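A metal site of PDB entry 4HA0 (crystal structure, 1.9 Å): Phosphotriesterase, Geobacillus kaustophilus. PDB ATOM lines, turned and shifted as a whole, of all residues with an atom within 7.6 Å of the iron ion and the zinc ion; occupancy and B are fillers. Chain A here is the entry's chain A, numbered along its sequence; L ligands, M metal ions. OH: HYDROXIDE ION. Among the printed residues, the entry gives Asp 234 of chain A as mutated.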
ATOM      1  N   HIS A  27     -18.717  18.596  20.139  1.00  0.00           N
ATOM      2  CA  HIS A  27     -17.759  19.203  21.056  1.00  0.00           C
ATOM      3  C   HIS A  27     -16.536  18.321  21.360  1.00  0.00           C
ATOM      4  O   HIS A  27     -16.618  17.442  22.208  1.00  0.00           O
ATOM      5  CB  HIS A  27     -18.464  19.551  22.377  1.00  0.00           C
ATOM      6  CG  HIS A  27     -17.739  20.551  23.220  1.00  0.00           C
ATOM      7  ND1 HIS A  27     -18.364  21.686  23.695  1.00  0.00           N
ATOM      8  CD2 HIS A  27     -16.482  20.587  23.706  1.00  0.00           C
ATOM      9  CE1 HIS A  27     -17.516  22.390  24.426  1.00  0.00           C
ATOM     10  NE2 HIS A  27     -16.364  21.750  24.436  1.00  0.00           N
ATOM     11  N   GLU A  28     -15.427  18.566  20.657  1.00  0.00           N
ATOM     12  CA  GLU A  28     -14.145  17.894  20.901  1.00  0.00           C
ATOM     13  C   GLU A  28     -13.014  18.888  20.637  1.00  0.00           C
ATOM     14  O   GLU A  28     -13.210  19.826  19.849  1.00  0.00           O
ATOM     15  CB  GLU A  28     -13.993  16.678  19.987  1.00  0.00           C
ATOM     16  CG  GLU A  28     -15.221  15.759  19.901  1.00  0.00           C
ATOM     17  CD  GLU A  28     -15.354  14.825  21.092  1.00  0.00           C
ATOM     18  OE1 GLU A  28     -14.349  14.626  21.809  1.00  0.00           O
ATOM     19  OE2 GLU A  28     -16.470  14.289  21.312  1.00  0.00           O
ATOM     20  N   HIS A  29     -11.849  18.709  21.280  1.00  0.00           N
ATOM     21  CA  HIS A  29     -10.656  19.523  20.989  1.00  0.00           C
ATOM     22  C   HIS A  29      -9.524  18.702  20.420  1.00  0.00           C
ATOM     23  O   HIS A  29      -9.044  17.767  21.081  1.00  0.00           O
ATOM     24  CB  HIS A  29     -10.115  20.186  22.262  1.00  0.00           C
ATOM     25  CG  HIS A  29     -11.104  21.051  22.942  1.00  0.00           C
ATOM     26  ND1 HIS A  29     -11.233  22.389  22.654  1.00  0.00           N
ATOM     27  CD2 HIS A  29     -12.017  20.784  23.904  1.00  0.00           C
ATOM     28  CE1 HIS A  29     -12.204  22.905  23.380  1.00  0.00           C
ATOM     29  NE2 HIS A  29     -12.686  21.956  24.158  1.00  0.00           N
ATOM     30  N   PHE A  32      -5.645  21.738  22.891  1.00  0.00           N
ATOM     31  CA  PHE A  32      -6.120  22.605  23.978  1.00  0.00           C
ATOM     32  C   PHE A  32      -4.980  22.904  24.961  1.00  0.00           C
ATOM     33  O   PHE A  32      -4.273  22.003  25.374  1.00  0.00           O
ATOM     34  CB  PHE A  32      -7.268  21.968  24.747  1.00  0.00           C
ATOM     35  CG  PHE A  32      -7.918  22.889  25.758  1.00  0.00           C
ATOM     36  CD1 PHE A  32      -7.385  23.028  27.043  1.00  0.00           C
ATOM     37  CD2 PHE A  32      -9.070  23.602  25.431  1.00  0.00           C
ATOM     38  CE1 PHE A  32      -7.972  23.876  27.986  1.00  0.00           C
ATOM     39  CE2 PHE A  32      -9.664  24.459  26.368  1.00  0.00           C
ATOM     40  CZ  PHE A  32      -9.126  24.597  27.644  1.00  0.00           C
ATOM     41  N   ASP A  72     -15.117  21.956  16.804  1.00  0.00           N
ATOM     42  CA  ASP A  72     -14.006  22.160  17.738  1.00  0.00           C
ATOM     43  C   ASP A  72     -14.080  23.585  18.264  1.00  0.00           C
ATOM     44  O   ASP A  72     -13.686  24.521  17.577  1.00  0.00           O
ATOM     45  CB  ASP A  72     -12.681  21.922  17.021  1.00  0.00           C
ATOM     46  CG  ASP A  72     -11.462  22.067  17.946  1.00  0.00           C
ATOM     47  OD1 ASP A  72     -11.557  22.831  18.922  1.00  0.00           O
ATOM     48  OD2 ASP A  72     -10.438  21.422  17.682  1.00  0.00           O
ATOM     49  N   PRO A  73     -14.602  23.755  19.488  1.00  0.00           N
ATOM     50  CA  PRO A  73     -14.840  25.093  20.037  1.00  0.00           C
ATOM     51  C   PRO A  73     -13.729  25.532  20.991  1.00  0.00           C
ATOM     52  O   PRO A  73     -14.016  26.185  22.014  1.00  0.00           O
ATOM     53  CB  PRO A  73     -16.119  24.893  20.832  1.00  0.00           C
ATOM     54  CG  PRO A  73     -15.951  23.497  21.410  1.00  0.00           C
ATOM     55  CD  PRO A  73     -15.147  22.713  20.373  1.00  0.00           C
ATOM     56  N   THR A  74     -12.491  25.169  20.677  1.00  0.00           N
ATOM     57  CA  THR A  74     -11.350  25.643  21.443  1.00  0.00           C
ATOM     58  C   THR A  74     -11.373  27.173  21.466  1.00  0.00           C
ATOM     59  O   THR A  74     -11.418  27.805  20.420  1.00  0.00           O
ATOM     60  CB  THR A  74     -10.016  25.174  20.828  1.00  0.00           C
ATOM     61  OG1 THR A  74      -9.993  23.737  20.743  1.00  0.00           O
ATOM     62  CG2 THR A  74      -8.843  25.674  21.655  1.00  0.00           C
ATOM     63  N   PRO A  75     -11.407  27.759  22.672  1.00  0.00           N
ATOM     64  CA  PRO A  75     -11.418  29.218  22.854  1.00  0.00           C
ATOM     65  C   PRO A  75     -10.178  29.893  22.286  1.00  0.00           C
ATOM     66  O   PRO A  75      -9.113  29.301  22.307  1.00  0.00           O
ATOM     67  CB  PRO A  75     -11.414  29.377  24.388  1.00  0.00           C
ATOM     68  CG  PRO A  75     -12.038  28.114  24.913  1.00  0.00           C
ATOM     69  CD  PRO A  75     -11.569  27.031  23.952  1.00  0.00           C
ATOM     70  N   TYR A 103     -12.608  31.932  26.845  1.00  0.00           N
ATOM     71  CA  TYR A 103     -13.038  31.055  27.910  1.00  0.00           C
ATOM     72  C   TYR A 103     -13.603  31.809  29.093  1.00  0.00           C
ATOM     73  O   TYR A 103     -13.632  33.003  29.087  1.00  0.00           O
ATOM     74  CB  TYR A 103     -11.895  30.170  28.390  1.00  0.00           C
ATOM     75  CG  TYR A 103     -12.181  28.731  28.674  1.00  0.00           C
ATOM     76  CD1 TYR A 103     -13.255  28.067  28.131  1.00  0.00           C
ATOM     77  CD2 TYR A 103     -11.361  28.025  29.507  1.00  0.00           C
ATOM     78  CE1 TYR A 103     -13.468  26.751  28.390  1.00  0.00           C
ATOM     79  CE2 TYR A 103     -11.593  26.712  29.779  1.00  0.00           C
ATOM     80  CZ  TYR A 103     -12.642  26.074  29.212  1.00  0.00           C
ATOM     81  OH  TYR A 103     -12.858  24.756  29.458  1.00  0.00           O
ATOM     82  N   TYR A 104     -14.077  31.054  30.054  1.00  0.00           N
ATOM     83  CA  TYR A 104     -14.626  31.609  31.267  1.00  0.00           C
ATOM     84  C   TYR A 104     -13.549  32.240  32.122  1.00  0.00           C
ATOM     85  O   TYR A 104     -12.438  31.946  31.967  1.00  0.00           O
ATOM     86  CB  TYR A 104     -15.465  30.616  32.042  1.00  0.00           C
ATOM     87  CG  TYR A 104     -14.762  29.552  32.855  1.00  0.00           C
ATOM     88  CD1 TYR A 104     -14.345  28.391  32.299  1.00  0.00           C
ATOM     89  CD2 TYR A 104     -14.608  29.711  34.232  1.00  0.00           C
ATOM     90  CE1 TYR A 104     -13.755  27.450  33.049  1.00  0.00           C
ATOM     91  CE2 TYR A 104     -14.028  28.749  34.979  1.00  0.00           C
ATOM     92  CZ  TYR A 104     -13.601  27.634  34.386  1.00  0.00           C
ATOM     93  OH  TYR A 104     -13.039  26.685  35.144  1.00  0.00           O
ATOM     94  N   KCX A 149     -18.153  30.642  20.584  1.00  0.00           N
ATOM     95  CA  KCX A 149     -18.043  29.943  21.855  1.00  0.00           C
ATOM     96  CB  KCX A 149     -16.695  29.227  21.947  1.00  0.00           C
ATOM     97  CG  KCX A 149     -16.338  28.654  23.330  1.00  0.00           C
ATOM     98  CD  KCX A 149     -17.394  27.682  23.822  1.00  0.00           C
ATOM     99  CE  KCX A 149     -16.861  26.809  24.925  1.00  0.00           C
ATOM    100  NZ  KCX A 149     -15.625  26.064  24.557  1.00  0.00           N
ATOM    101  C   KCX A 149     -18.235  30.911  23.034  1.00  0.00           C
ATOM    102  O   KCX A 149     -17.550  31.933  23.135  1.00  0.00           O
ATOM    103  CX  KCX A 149     -15.307  24.988  25.275  1.00  0.00           C
ATOM    104  OQ1 KCX A 149     -14.292  24.318  25.046  1.00  0.00           O
ATOM    105  OQ2 KCX A 149     -16.063  24.672  26.185  1.00  0.00           O
ATOM    106  N   LEU A 150     -19.177  30.584  23.906  1.00  0.00           N
ATOM    107  CA  LEU A 150     -19.368  31.347  25.143  1.00  0.00           C
ATOM    108  C   LEU A 150     -19.050  30.476  26.377  1.00  0.00           C
ATOM    109  O   LEU A 150     -19.194  29.257  26.321  1.00  0.00           O
ATOM    110  CB  LEU A 150     -20.800  31.870  25.234  1.00  0.00           C
ATOM    111  CG  LEU A 150     -21.225  32.963  24.262  1.00  0.00           C
ATOM    112  CD1 LEU A 150     -22.687  33.370  24.543  1.00  0.00           C
ATOM    113  CD2 LEU A 150     -20.286  34.159  24.367  1.00  0.00           C
ATOM    114  N   ALA A 151     -18.625  31.095  27.472  1.00  0.00           N
ATOM    115  CA  ALA A 151     -18.312  30.308  28.654  1.00  0.00           C
ATOM    116  C   ALA A 151     -18.628  31.103  29.905  1.00  0.00           C
ATOM    117  O   ALA A 151     -18.433  32.324  29.933  1.00  0.00           O
ATOM    118  CB  ALA A 151     -16.845  29.902  28.622  1.00  0.00           C
ATOM    119  N   THR A 181     -22.066  26.867  24.133  1.00  0.00           N
ATOM    120  CA  THR A 181     -21.589  27.346  25.435  1.00  0.00           C
ATOM    121  C   THR A 181     -20.896  26.285  26.265  1.00  0.00           C
ATOM    122  O   THR A 181     -21.047  25.095  26.024  1.00  0.00           O
ATOM    123  CB  THR A 181     -22.720  27.929  26.278  1.00  0.00           C
ATOM    124  OG1 THR A 181     -23.468  26.869  26.895  1.00  0.00           O
ATOM    125  CG2 THR A 181     -23.652  28.741  25.419  1.00  0.00           C
ATOM    126  N   HIS A 182     -20.125  26.764  27.246  1.00  0.00           N
ATOM    127  CA  HIS A 182     -19.574  25.948  28.339  1.00  0.00           C
ATOM    128  C   HIS A 182     -20.251  26.373  29.651  1.00  0.00           C
ATOM    129  O   HIS A 182     -20.321  27.570  29.972  1.00  0.00           O
ATOM    130  CB  HIS A 182     -18.057  26.148  28.422  1.00  0.00           C
ATOM    131  CG  HIS A 182     -17.458  25.949  29.791  1.00  0.00           C
ATOM    132  ND1 HIS A 182     -16.561  24.948  30.076  1.00  0.00           N
ATOM    133  CD2 HIS A 182     -17.597  26.657  30.939  1.00  0.00           C
ATOM    134  CE1 HIS A 182     -16.173  25.034  31.332  1.00  0.00           C
ATOM    135  NE2 HIS A 182     -16.788  26.058  31.889  1.00  0.00           N
ATOM    136  N   THR A 183     -20.764  25.413  30.402  1.00  0.00           N
ATOM    137  CA  THR A 183     -21.232  25.706  31.753  1.00  0.00           C
ATOM    138  C   THR A 183     -20.288  25.082  32.751  1.00  0.00           C
ATOM    139  O   THR A 183     -19.793  23.978  32.535  1.00  0.00           O
ATOM    140  CB  THR A 183     -22.690  25.212  32.023  1.00  0.00           C
ATOM    141  OG1 THR A 183     -22.796  23.793  31.764  1.00  0.00           O
ATOM    142  CG2 THR A 183     -23.662  25.967  31.173  1.00  0.00           C
ATOM    143  N   GLN A 184     -20.035  25.776  33.861  1.00  0.00           N
ATOM    144  CA  GLN A 184     -19.039  25.274  34.811  1.00  0.00           C
ATOM    145  C   GLN A 184     -19.696  24.513  35.947  1.00  0.00           C
ATOM    146  O   GLN A 184     -20.631  25.007  36.593  1.00  0.00           O
ATOM    147  CB  GLN A 184     -18.184  26.429  35.354  1.00  0.00           C
ATOM    148  CG  GLN A 184     -17.068  25.977  36.295  1.00  0.00           C
ATOM    149  CD  GLN A 184     -15.943  25.229  35.581  1.00  0.00           C
ATOM    150  OE1 GLN A 184     -15.816  25.280  34.358  1.00  0.00           O
ATOM    151  NE2 GLN A 184     -15.114  24.535  36.360  1.00  0.00           N
ATOM    152  N   GLY A 209     -23.800  23.904  26.740  1.00  0.00           N
ATOM    153  CA  GLY A 209     -22.901  22.773  26.883  1.00  0.00           C
ATOM    154  C   GLY A 209     -22.724  22.288  28.298  1.00  0.00           C
ATOM    155  O   GLY A 209     -23.135  22.953  29.258  1.00  0.00           O
ATOM    156  N   HIS A 210     -22.101  21.117  28.438  1.00  0.00           N
ATOM    157  CA  HIS A 210     -21.765  20.536  29.740  1.00  0.00           C
ATOM    158  C   HIS A 210     -22.970  20.437  30.666  1.00  0.00           C
ATOM    159  O   HIS A 210     -22.851  20.569  31.886  1.00  0.00           O
ATOM    160  CB  HIS A 210     -20.633  21.321  30.402  1.00  0.00           C
ATOM    161  CG  HIS A 210     -19.471  21.536  29.490  1.00  0.00           C
ATOM    162  ND1 HIS A 210     -19.232  20.718  28.408  1.00  0.00           N
ATOM    163  CD2 HIS A 210     -18.504  22.481  29.466  1.00  0.00           C
ATOM    164  CE1 HIS A 210     -18.161  21.135  27.772  1.00  0.00           C
ATOM    165  NE2 HIS A 210     -17.708  22.198  28.387  1.00  0.00           N
ATOM    166  N   ASP A 233     -21.840  16.513  26.575  1.00  0.00           N
ATOM    167  CA  ASP A 233     -20.620  16.553  25.761  1.00  0.00           C
ATOM    168  C   ASP A 233     -19.350  16.189  26.520  1.00  0.00           C
ATOM    169  O   ASP A 233     -18.249  16.364  25.989  1.00  0.00           O
ATOM    170  CB  ASP A 233     -20.477  17.957  25.188  1.00  0.00           C
ATOM    171  CG  ASP A 233     -20.644  19.030  26.246  1.00  0.00           C
ATOM    172  OD1 ASP A 233     -20.438  18.737  27.435  1.00  0.00           O
ATOM    173  OD2 ASP A 233     -21.015  20.163  25.873  1.00  0.00           O
ATOM    174  N   ASP A 234     -19.492  15.704  27.748  1.00  0.00           N
ATOM    175  CA  ASP A 234     -18.349  15.409  28.585  1.00  0.00           C
ATOM    176  C   ASP A 234     -18.175  13.914  28.856  1.00  0.00           C
ATOM    177  O   ASP A 234     -17.571  13.539  29.859  1.00  0.00           O
ATOM    178  CB  ASP A 234     -18.484  16.133  29.943  1.00  0.00           C
ATOM    179  CG  ASP A 234     -17.922  17.543  29.919  1.00  0.00           C
ATOM    180  OD1 ASP A 234     -17.024  17.809  29.102  1.00  0.00           O
ATOM    181  OD2 ASP A 234     -18.392  18.375  30.723  1.00  0.00           O
ATOM    182  N   HIS A 269     -17.620  14.107  23.725  1.00  0.00           N
ATOM    183  CA  HIS A 269     -16.676  13.763  24.782  1.00  0.00           C
ATOM    184  C   HIS A 269     -15.909  14.931  25.376  1.00  0.00           C
ATOM    185  O   HIS A 269     -15.404  14.809  26.490  1.00  0.00           O
ATOM    186  CB  HIS A 269     -15.640  12.775  24.278  1.00  0.00           C
ATOM    187  CG  HIS A 269     -16.214  11.597  23.553  1.00  0.00           C
ATOM    188  ND1 HIS A 269     -16.373  11.591  22.184  1.00  0.00           N
ATOM    189  CD2 HIS A 269     -16.626  10.389  23.994  1.00  0.00           C
ATOM    190  CE1 HIS A 269     -16.864  10.419  21.811  1.00  0.00           C
ATOM    191  NE2 HIS A 269     -17.026   9.676  22.895  1.00  0.00           N
ATOM    192  N   ASP A 270     -15.797  16.034  24.636  1.00  0.00           N
ATOM    193  CA  ASP A 270     -14.959  17.156  25.069  1.00  0.00           C
ATOM    194  C   ASP A 270     -13.494  16.712  25.219  1.00  0.00           C
ATOM    195  O   ASP A 270     -12.777  17.221  26.093  1.00  0.00           O
ATOM    196  CB  ASP A 270     -15.486  17.694  26.403  1.00  0.00           C
ATOM    197  CG  ASP A 270     -14.931  19.059  26.747  1.00  0.00           C
ATOM    198  OD1 ASP A 270     -14.350  19.684  25.858  1.00  0.00           O
ATOM    199  OD2 ASP A 270     -15.084  19.496  27.896  1.00  0.00           O
ATOM    200  N   THR A 271     -13.048  15.759  24.398  1.00  0.00           N
ATOM    201  CA  THR A 271     -11.657  15.280  24.475  1.00  0.00           C
ATOM    202  C   THR A 271     -10.652  16.395  24.210  1.00  0.00           C
ATOM    203  O   THR A 271     -10.961  17.385  23.535  1.00  0.00           O
ATOM    204  CB  THR A 271     -11.356  14.135  23.484  1.00  0.00           C
ATOM    205  OG1 THR A 271     -11.568  14.559  22.129  1.00  0.00           O
ATOM    206  CG2 THR A 271     -12.185  12.898  23.767  1.00  0.00           C
ATOM    207  N   VAL A 272      -9.433  16.225  24.720  1.00  0.00           N
ATOM    208  CA  VAL A 272      -8.304  17.032  24.321  1.00  0.00           C
ATOM    209  C   VAL A 272      -7.296  16.046  23.825  1.00  0.00           C
ATOM    210  O   VAL A 272      -6.846  15.204  24.557  1.00  0.00           O
ATOM    211  CB  VAL A 272      -7.694  17.818  25.497  1.00  0.00           C
ATOM    212  CG1 VAL A 272      -6.515  18.620  25.012  1.00  0.00           C
ATOM    213  CG2 VAL A 272      -8.720  18.728  26.101  1.00  0.00           C
HETATM  214  O    OH L   1     -14.233  22.017  27.879  1.00  0.00           O
HETATM  215 FE    FE M   1     -14.445  22.053  25.593  1.00  0.00          FE
HETATM  216 ZN    ZN M   2     -15.972  23.639  28.180  1.00  0.00          ZN
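The backbone carbonyl oxygen (O) of Pro 73 is in hydrogen-bond range of NZ of KCX 149 (3.0 Å).
A ring nitrogen (ND1) of His 210 sits at hydrogen-bond distance from the side-chain carboxylate (OD2) of Asp 234 (3.4 Å).
OD1 of Asp 233 lies within hydrogen-bond range of ND1 of His 210.
OG1 of Thr 74 sits at hydrogen-bond distance from ND1 of His 29, at 2.6 Å.
OE1 of Gln 184 sits at hydrogen-bond distance from NE2 of His 182 (2.8 Å).
The backbone NH of His 182 lies within hydrogen-bond range of the backbone carbonyl oxygen of Leu 150, 2.8 Å away.
OE1 of Glu 28 lies within hydrogen-bond range of N of Asp 270, 3.5 Å away.
The backbone carbonyl oxygen (O) of Asp 233 is in hydrogen-bond range of the backbone NH (N) of Asp 270 (2.8 Å).
Four residues have an atom within 4 Å of the iron ion: His 27, His 29, KCX 149 and Asp 270.
Residues that only touch the zinc ion: Tyr 103 (3.5 Å).
Within 4 Å of the zinc ion: Tyr 103, KCX 149, His 182 and His 210.
The nearest printed residue that does not touch the zinc ion is His 27 (4.2 Å).
The iron ion is bound by NE2 of His 27 (2.3 Å), NE2 of His 29 (2.3 Å), O of the ligand (2.3 Å), OQ1 of KCX 149 (2.3 Å) and OD1 of Asp 270 (2.4 Å).
The iron ion has five donor atoms within binding distance.
The zinc ion is bound by OQ2 of KCX 149 (2.2 Å), a ring nitrogen (NE2) of His 210 (2.3 Å), a ring nitrogen (ND1) of His 182 (2.4 Å) and an oxygen (O) of the ligand (2.4 Å).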
